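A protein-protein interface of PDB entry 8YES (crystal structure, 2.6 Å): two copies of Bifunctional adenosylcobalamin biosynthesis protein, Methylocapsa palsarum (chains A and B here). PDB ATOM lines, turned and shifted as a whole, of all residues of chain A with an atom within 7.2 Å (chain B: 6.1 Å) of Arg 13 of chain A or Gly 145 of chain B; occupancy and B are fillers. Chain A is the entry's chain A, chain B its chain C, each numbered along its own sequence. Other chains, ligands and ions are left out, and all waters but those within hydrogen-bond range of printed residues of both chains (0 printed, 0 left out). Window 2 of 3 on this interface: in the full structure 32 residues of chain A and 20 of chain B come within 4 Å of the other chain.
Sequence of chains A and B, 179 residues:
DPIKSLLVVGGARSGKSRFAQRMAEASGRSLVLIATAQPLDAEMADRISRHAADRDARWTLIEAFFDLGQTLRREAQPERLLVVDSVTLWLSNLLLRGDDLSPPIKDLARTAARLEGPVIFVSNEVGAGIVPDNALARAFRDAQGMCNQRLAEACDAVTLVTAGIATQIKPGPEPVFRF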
ATOM      1  N   GLY A  10       4.470  12.339  29.549  1.00  0.00           N
ATOM      2  CA  GLY A  10       4.551  10.905  29.210  1.00  0.00           C
ATOM      3  C   GLY A  10       5.732  10.532  28.328  1.00  0.00           C
ATOM      4  O   GLY A  10       6.429  11.414  27.815  1.00  0.00           O
ATOM      5  N   GLY A  11       5.929   9.231  28.125  1.00  0.00           N
ATOM      6  CA  GLY A  11       6.979   8.641  27.281  1.00  0.00           C
ATOM      7  C   GLY A  11       6.665   8.906  25.827  1.00  0.00           C
ATOM      8  O   GLY A  11       5.640   9.531  25.577  1.00  0.00           O
ATOM      9  N   ALA A  12       7.504   8.437  24.911  1.00  0.00           N
ATOM     10  CA  ALA A  12       7.276   8.519  23.455  1.00  0.00           C
ATOM     11  C   ALA A  12       6.079   7.647  23.059  1.00  0.00           C
ATOM     12  O   ALA A  12       6.034   6.460  23.418  1.00  0.00           O
ATOM     13  CB  ALA A  12       8.532   8.110  22.703  1.00  0.00           C
ATOM     14  N   ARG A  13       5.176   8.208  22.266  1.00  0.00           N
ATOM     15  CA  ARG A  13       3.970   7.521  21.733  1.00  0.00           C
ATOM     16  C   ARG A  13       3.198   6.949  22.925  1.00  0.00           C
ATOM     17  O   ARG A  13       2.872   5.786  22.897  1.00  0.00           O
ATOM     18  CB  ARG A  13       4.338   6.476  20.672  1.00  0.00           C
ATOM     19  CG  ARG A  13       4.341   7.008  19.246  1.00  0.00           C
ATOM     20  CD  ARG A  13       2.963   7.037  18.589  1.00  0.00           C
ATOM     21  NE  ARG A  13       3.033   7.194  17.131  1.00  0.00           N
ATOM     22  CZ  ARG A  13       3.351   8.321  16.489  1.00  0.00           C
ATOM     23  NH1 ARG A  13       3.634   9.437  17.148  1.00  0.00           N
ATOM     24  NH2 ARG A  13       3.389   8.327  15.170  1.00  0.00           N
ATOM     25  N   SER A  14       2.950   7.784  23.926  1.00  0.00           N
ATOM     26  CA  SER A  14       2.201   7.509  25.176  1.00  0.00           C
ATOM     27  C   SER A  14       0.726   7.925  25.024  1.00  0.00           C
ATOM     28  O   SER A  14      -0.049   7.578  25.900  1.00  0.00           O
ATOM     29  CB  SER A  14       2.847   8.238  26.332  1.00  0.00           C
ATOM     30  OG  SER A  14       2.873   9.653  26.106  1.00  0.00           O
ATOM     31  N   GLY A  15       0.371   8.688  23.993  1.00  0.00           N
ATOM     32  CA  GLY A  15      -0.934   9.365  23.845  1.00  0.00           C
ATOM     33  C   GLY A  15      -1.054  10.733  24.539  1.00  0.00           C
ATOM     34  O   GLY A  15      -2.190  11.207  24.696  1.00  0.00           O
ATOM     35  N   LYS A  16       0.035  11.407  24.913  1.00  0.00           N
ATOM     36  CA  LYS A  16      -0.072  12.706  25.638  1.00  0.00           C
ATOM     37  C   LYS A  16      -0.633  13.831  24.738  1.00  0.00           C
ATOM     38  O   LYS A  16      -1.374  14.653  25.276  1.00  0.00           O
ATOM     39  CB  LYS A  16       1.265  13.085  26.279  1.00  0.00           C
ATOM     40  CG  LYS A  16       2.447  13.229  25.333  1.00  0.00           C
ATOM     41  CD  LYS A  16       3.802  13.124  26.042  1.00  0.00           C
ATOM     42  CE  LYS A  16       4.950  13.613  25.186  1.00  0.00           C
ATOM     43  NZ  LYS A  16       5.432  12.582  24.238  1.00  0.00           N
ATOM     44  N   ARG A  47       5.453  12.973  11.179  1.00  0.00           N
ATOM     45  CA  ARG A  47       4.780  13.118  12.512  1.00  0.00           C
ATOM     46  C   ARG A  47       4.060  14.482  12.619  1.00  0.00           C
ATOM     47  O   ARG A  47       3.027  14.530  13.323  1.00  0.00           O
ATOM     48  CB  ARG A  47       5.769  12.967  13.683  1.00  0.00           C
ATOM     49  CG  ARG A  47       5.306  12.118  14.873  1.00  0.00           C
ATOM     50  CD  ARG A  47       6.038  10.779  14.952  1.00  0.00           C
ATOM     51  NE  ARG A  47       6.371  10.266  16.279  1.00  0.00           N
ATOM     52  CZ  ARG A  47       7.361  10.704  17.055  1.00  0.00           C
ATOM     53  NH1 ARG A  47       8.116  11.730  16.701  1.00  0.00           N
ATOM     54  NH2 ARG A  47       7.576  10.124  18.219  1.00  0.00           N
ATOM     55  N   ARG A  50       0.617  14.389   9.981  1.00  0.00           N
ATOM     56  CA  ARG A  50      -0.567  13.632  10.495  1.00  0.00           C
ATOM     57  C   ARG A  50      -1.234  14.476  11.591  1.00  0.00           C
ATOM     58  O   ARG A  50      -2.480  14.526  11.600  1.00  0.00           O
ATOM     59  CB  ARG A  50      -0.194  12.230  11.001  1.00  0.00           C
ATOM     60  CG  ARG A  50       0.598  11.378  10.015  1.00  0.00           C
ATOM     61  CD  ARG A  50      -0.029  11.202   8.637  1.00  0.00           C
ATOM     62  NE  ARG A  50       0.855  11.701   7.583  1.00  0.00           N
ATOM     63  CZ  ARG A  50       0.661  12.801   6.842  1.00  0.00           C
ATOM     64  NH1 ARG A  50      -0.420  13.551   6.992  1.00  0.00           N
ATOM     65  NH2 ARG A  50       1.561  13.147   5.934  1.00  0.00           N
ATOM     66  N   HIS A  51      -0.428  15.119  12.454  1.00  0.00           N
ATOM     67  CA  HIS A  51      -0.843  16.113  13.490  1.00  0.00           C
ATOM     68  C   HIS A  51      -1.634  17.260  12.835  1.00  0.00           C
ATOM     69  O   HIS A  51      -2.647  17.684  13.429  1.00  0.00           O
ATOM     70  CB  HIS A  51       0.368  16.665  14.279  1.00  0.00           C
ATOM     71  CG  HIS A  51       0.676  15.963  15.564  1.00  0.00           C
ATOM     72  ND1 HIS A  51       1.974  15.643  15.939  1.00  0.00           N
ATOM     73  CD2 HIS A  51      -0.123  15.529  16.566  1.00  0.00           C
ATOM     74  CE1 HIS A  51       1.958  15.032  17.105  1.00  0.00           C
ATOM     75  NE2 HIS A  51       0.683  14.950  17.511  1.00  0.00           N
ATOM     76  N   ASN A 124       7.912  15.340  27.740  1.00  0.00           N
ATOM     77  CA  ASN A 124       8.349  13.934  27.807  1.00  0.00           C
ATOM     78  C   ASN A 124       9.027  13.682  29.155  1.00  0.00           C
ATOM     79  O   ASN A 124       9.736  14.570  29.652  1.00  0.00           O
ATOM     80  CB  ASN A 124       9.290  13.590  26.656  1.00  0.00           C
ATOM     81  CG  ASN A 124       8.576  13.407  25.334  1.00  0.00           C
ATOM     82  OD1 ASN A 124       8.627  12.344  24.751  1.00  0.00           O
ATOM     83  ND2 ASN A 124       7.928  14.440  24.832  1.00  0.00           N
ATOM     84  N   THR A 162       0.033   7.152  30.442  1.00  0.00           N
ATOM     85  CA  THR A 162       0.588   5.826  30.073  1.00  0.00           C
ATOM     86  C   THR A 162      -0.391   5.091  29.156  1.00  0.00           C
ATOM     87  O   THR A 162      -1.597   5.063  29.472  1.00  0.00           O
ATOM     88  CB  THR A 162       0.859   4.950  31.297  1.00  0.00           C
ATOM     89  OG1 THR A 162       1.528   5.719  32.292  1.00  0.00           O
ATOM     90  CG2 THR A 162       1.712   3.744  30.959  1.00  0.00           C
ATOM     91  N   ALA A 163       0.118   4.528  28.058  1.00  0.00           N
ATOM     92  CA  ALA A 163      -0.631   3.640  27.148  1.00  0.00           C
ATOM     93  C   ALA A 163      -1.964   4.286  26.770  1.00  0.00           C
ATOM     94  O   ALA A 163      -2.992   3.573  26.685  1.00  0.00           O
ATOM     95  CB  ALA A 163      -0.822   2.313  27.842  1.00  0.00           C
ATOM     96  N   GLY A 164      -1.953   5.599  26.566  1.00  0.00           N
ATOM     97  CA  GLY A 164      -3.116   6.391  26.086  1.00  0.00           C
ATOM     98  C   GLY A 164      -4.052   6.814  27.203  1.00  0.00           C
ATOM     99  O   GLY A 164      -5.112   7.345  26.888  1.00  0.00           O
ATOM    100  N   GLU B 125       6.869  -1.212  28.861  1.00  0.00           N
ATOM    101  CA  GLU B 125       7.013   0.226  28.524  1.00  0.00           C
ATOM    102  C   GLU B 125       8.470   0.443  28.105  1.00  0.00           C
ATOM    103  O   GLU B 125       9.379   0.076  28.872  1.00  0.00           O
ATOM    104  CB  GLU B 125       6.620   1.124  29.693  1.00  0.00           C
ATOM    105  CG  GLU B 125       6.916   2.604  29.456  1.00  0.00           C
ATOM    106  CD  GLU B 125       6.003   3.371  28.496  1.00  0.00           C
ATOM    107  OE1 GLU B 125       6.554   4.141  27.630  1.00  0.00           O
ATOM    108  OE2 GLU B 125       4.737   3.234  28.631  1.00  0.00           O
ATOM    109  N   VAL B 126       8.687   1.025  26.933  1.00  0.00           N
ATOM    110  CA  VAL B 126      10.052   1.286  26.404  1.00  0.00           C
ATOM    111  C   VAL B 126      10.225   2.744  25.980  1.00  0.00           C
ATOM    112  O   VAL B 126      11.137   2.990  25.252  1.00  0.00           O
ATOM    113  CB  VAL B 126      10.308   0.321  25.241  1.00  0.00           C
ATOM    114  CG1 VAL B 126      10.124  -1.115  25.715  1.00  0.00           C
ATOM    115  CG2 VAL B 126       9.436   0.639  24.041  1.00  0.00           C
ATOM    116  N   PHE B 140      10.935   0.714  16.723  1.00  0.00           N
ATOM    117  CA  PHE B 140      10.360  -0.160  17.766  1.00  0.00           C
ATOM    118  C   PHE B 140       9.646   0.679  18.835  1.00  0.00           C
ATOM    119  O   PHE B 140       8.458   0.422  19.119  1.00  0.00           O
ATOM    120  CB  PHE B 140      11.417  -1.033  18.424  1.00  0.00           C
ATOM    121  CG  PHE B 140      10.795  -2.035  19.354  1.00  0.00           C
ATOM    122  CD1 PHE B 140      10.076  -3.094  18.852  1.00  0.00           C
ATOM    123  CD2 PHE B 140      10.905  -1.900  20.722  1.00  0.00           C
ATOM    124  CE1 PHE B 140       9.504  -4.023  19.705  1.00  0.00           C
ATOM    125  CE2 PHE B 140      10.350  -2.837  21.573  1.00  0.00           C
ATOM    126  CZ  PHE B 140       9.637  -3.890  21.063  1.00  0.00           C
ATOM    127  N   ARG B 141      10.332   1.673  19.384  1.00  0.00           N
ATOM    128  CA  ARG B 141       9.784   2.579  20.435  1.00  0.00           C
ATOM    129  C   ARG B 141       8.385   3.139  20.092  1.00  0.00           C
ATOM    130  O   ARG B 141       7.574   3.237  21.005  1.00  0.00           O
ATOM    131  CB  ARG B 141      10.730   3.752  20.654  1.00  0.00           C
ATOM    132  CG  ARG B 141      10.586   4.303  22.054  1.00  0.00           C
ATOM    133  CD  ARG B 141      11.813   5.061  22.466  1.00  0.00           C
ATOM    134  NE  ARG B 141      11.798   6.380  21.854  1.00  0.00           N
ATOM    135  CZ  ARG B 141      12.023   7.508  22.498  1.00  0.00           C
ATOM    136  NH1 ARG B 141      12.305   7.502  23.792  1.00  0.00           N
ATOM    137  NH2 ARG B 141      11.988   8.642  21.827  1.00  0.00           N
ATOM    138  N   ASP B 142       8.141   3.479  18.828  1.00  0.00           N
ATOM    139  CA  ASP B 142       6.840   3.935  18.265  1.00  0.00           C
ATOM    140  C   ASP B 142       5.838   2.782  18.185  1.00  0.00           C
ATOM    141  O   ASP B 142       4.666   2.985  18.551  1.00  0.00           O
ATOM    142  CB  ASP B 142       6.957   4.465  16.826  1.00  0.00           C
ATOM    143  CG  ASP B 142       7.419   5.899  16.725  1.00  0.00           C
ATOM    144  OD1 ASP B 142       8.533   6.156  17.168  1.00  0.00           O
ATOM    145  OD2 ASP B 142       6.628   6.757  16.249  1.00  0.00           O
ATOM    146  N   ALA B 143       6.246   1.643  17.634  1.00  0.00           N
ATOM    147  CA  ALA B 143       5.339   0.483  17.506  1.00  0.00           C
ATOM    148  C   ALA B 143       4.915   0.040  18.917  1.00  0.00           C
ATOM    149  O   ALA B 143       3.742  -0.145  19.128  1.00  0.00           O
ATOM    150  CB  ALA B 143       5.999  -0.619  16.723  1.00  0.00           C
ATOM    151  N   GLN B 144       5.836  -0.013  19.874  1.00  0.00           N
ATOM    152  CA  GLN B 144       5.546  -0.463  21.258  1.00  0.00           C
ATOM    153  C   GLN B 144       4.548   0.474  21.931  1.00  0.00           C
ATOM    154  O   GLN B 144       3.631  -0.047  22.571  1.00  0.00           O
ATOM    155  CB  GLN B 144       6.815  -0.559  22.108  1.00  0.00           C
ATOM    156  CG  GLN B 144       6.548  -1.092  23.513  1.00  0.00           C
ATOM    157  CD  GLN B 144       6.034  -2.516  23.544  1.00  0.00           C
ATOM    158  OE1 GLN B 144       6.723  -3.430  23.993  1.00  0.00           O
ATOM    159  NE2 GLN B 144       4.798  -2.715  23.116  1.00  0.00           N
ATOM    160  N   GLY B 145       4.735   1.790  21.814  1.00  0.00           N
ATOM    161  CA  GLY B 145       3.836   2.819  22.377  1.00  0.00           C
ATOM    162  C   GLY B 145       2.457   2.808  21.720  1.00  0.00           C
ATOM    163  O   GLY B 145       1.451   2.830  22.436  1.00  0.00           O
ATOM    164  N   MET B 146       2.393   2.778  20.399  1.00  0.00           N
ATOM    165  CA  MET B 146       1.113   2.725  19.648  1.00  0.00           C
ATOM    166  C   MET B 146       0.375   1.444  20.067  1.00  0.00           C
ATOM    167  O   MET B 146      -0.834   1.523  20.415  1.00  0.00           O
ATOM    168  CB  MET B 146       1.380   2.740  18.139  1.00  0.00           C
ATOM    169  CG  MET B 146       0.149   2.564  17.277  1.00  0.00           C
ATOM    170  SD  MET B 146       0.650   1.976  15.624  1.00  0.00           S
ATOM    171  CE  MET B 146      -0.901   1.951  14.723  1.00  0.00           C
ATOM    172  N   CYS B 147       1.075   0.303  20.064  1.00  0.00           N
ATOM    173  CA  CYS B 147       0.481  -1.020  20.363  1.00  0.00           C
ATOM    174  C   CYS B 147      -0.127  -0.994  21.762  1.00  0.00           C
ATOM    175  O   CYS B 147      -1.282  -1.406  21.887  1.00  0.00           O
ATOM    176  CB  CYS B 147       1.491  -2.149  20.235  1.00  0.00           C
ATOM    177  SG  CYS B 147       0.743  -3.783  20.463  1.00  0.00           S
ATOM    178  N   ASN B 148       0.606  -0.502  22.766  1.00  0.00           N
ATOM    179  CA  ASN B 148       0.116  -0.387  24.169  1.00  0.00           C
ATOM    180  C   ASN B 148      -1.060   0.590  24.229  1.00  0.00           C
ATOM    181  O   ASN B 148      -1.954   0.370  25.062  1.00  0.00           O
ATOM    182  CB  ASN B 148       1.202   0.015  25.168  1.00  0.00           C
ATOM    183  CG  ASN B 148       2.106  -1.142  25.530  1.00  0.00           C
ATOM    184  OD1 ASN B 148       1.864  -2.281  25.122  1.00  0.00           O
ATOM    185  ND2 ASN B 148       3.175  -0.863  26.262  1.00  0.00           N
ATOM    186  N   GLN B 149      -1.094   1.610  23.372  1.00  0.00           N
ATOM    187  CA  GLN B 149      -2.294   2.487  23.263  1.00  0.00           C
ATOM    188  C   GLN B 149      -3.474   1.676  22.704  1.00  0.00           C
ATOM    189  O   GLN B 149      -4.556   1.713  23.298  1.00  0.00           O
ATOM    190  CB  GLN B 149      -2.015   3.734  22.429  1.00  0.00           C
ATOM    191  CG  GLN B 149      -1.550   4.928  23.251  1.00  0.00           C
ATOM    192  CD  GLN B 149      -1.199   6.051  22.311  1.00  0.00           C
ATOM    193  OE1 GLN B 149      -2.003   6.934  22.042  1.00  0.00           O
ATOM    194  NE2 GLN B 149      -0.013   5.985  21.743  1.00  0.00           N
ATOM    195  N   ARG B 150      -3.290   0.928  21.623  1.00  0.00           N
ATOM    196  CA  ARG B 150      -4.419   0.191  20.990  1.00  0.00           C
ATOM    197  C   ARG B 150      -4.896  -0.977  21.880  1.00  0.00           C
ATOM    198  O   ARG B 150      -6.123  -1.101  22.004  1.00  0.00           O
ATOM    199  CB  ARG B 150      -4.057  -0.123  19.541  1.00  0.00           C
ATOM    200  CG  ARG B 150      -4.060   1.128  18.671  1.00  0.00           C
ATOM    201  CD  ARG B 150      -3.496   0.869  17.298  1.00  0.00           C
ATOM    202  NE  ARG B 150      -3.874   1.909  16.352  1.00  0.00           N
ATOM    203  CZ  ARG B 150      -5.101   2.084  15.871  1.00  0.00           C
ATOM    204  NH1 ARG B 150      -6.114   1.296  16.223  1.00  0.00           N
ATOM    205  NH2 ARG B 150      -5.307   3.048  15.004  1.00  0.00           N
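The guanidinium group of Arg 13 of chain A lies within salt-bridge range of the side-chain carboxylate of Asp 142 of chain B (3.7 Å).
O of Arg 13 of chain A sits at hydrogen-bond distance from NE2 of Gln 149 of chain B.
The guanidinium group (NE) of Arg 47 of chain A is in salt-bridge range of the side-chain carboxylate (OD2) of Asp 142 of chain B, at 3.5 Å.
O of Arg 13 of chain A sits close to O of Gly 145 of chain B, 3.3 Å away.
ND1 of His 51 of chain A sits at hydrogen-bond distance from O of Arg 47 of chain A (3.0 Å).
The backbone carbonyl oxygen (O) of Gly 11 of chain A is in hydrogen-bond range of the side-chain hydroxyl (OG) of Ser 14 of chain A, at 2.8 Å.
O of Ser 14 of chain A lies within hydrogen-bond range of N of Gly 164 of chain A, 2.8 Å away.
Ala 12 of chain A touches Arg 141 of chain B (CB to CZ, 3.5 Å).
O of Arg 13 of chain A touches N of Met 146 of chain B, at 3.9 Å.
Ser 14 of chain A touches Gln 149 of chain B (C to CD, 3.8 Å).
CA of Gly 15 of chain A touches OE1 of Gln 149 of chain B, 3.2 Å away.
OE2 of Glu 125 of chain B touches CG2 of Thr 162 of chain A, 3.9 Å away.
O of Asn 148 of chain B touches CB of Ala 163 of chain A (3.6 Å).
C of Ala 163 of chain A touches CG of Gln 149 of chain B, at 3.6 Å.
Gly 164 of chain A touches Gln 149 of chain B.
Arg 13 of chain A touches four residues of chain B.
Gly 145 of chain B touches just one residue of chain A: Arg 13.
Printed residues of chain A within 4 Å of Asp 142 of chain B: Arg 13 and Arg 47.
Of the printed residues of chain B, Arg 47 of chain A touches Asp 142.
Of the printed residues of chain B, Gly 15 of chain A touches Gln 149 (3.2 Å).
Printed residues of chain A within 4 Å of Met 146 of chain B: Arg 13.
Ala 143 of chain B touches none of the printed residues of chain A.
Val 126 of chain B touches none of the printed residues of chain A.
The nearest printed residue of chain B that does not touch Thr 162 of chain A is Gln 149 of chain B (6.0 Å).
Printed residues of chain A that touch a printed residue of chain B: Ala 12, Arg 13, Ser 14, Gly 15, Arg 47, Thr 162, Ala 163 and Gly 164.
Hydrophobic or aromatic side chains of chain A within 4 Å of the printed part of chain B: Ala 12 and Ala 163.
Among the printed residues, Asp or Glu carboxylates within 4 Å of a Lys or Arg side-chain nitrogen of the other chain: Arg 13 of chain A with Asp 142 of chain B (3.7 Å) and Arg 47 of chain A with Asp 142 of chain B (3.5 Å).
No position is printed for both chains.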
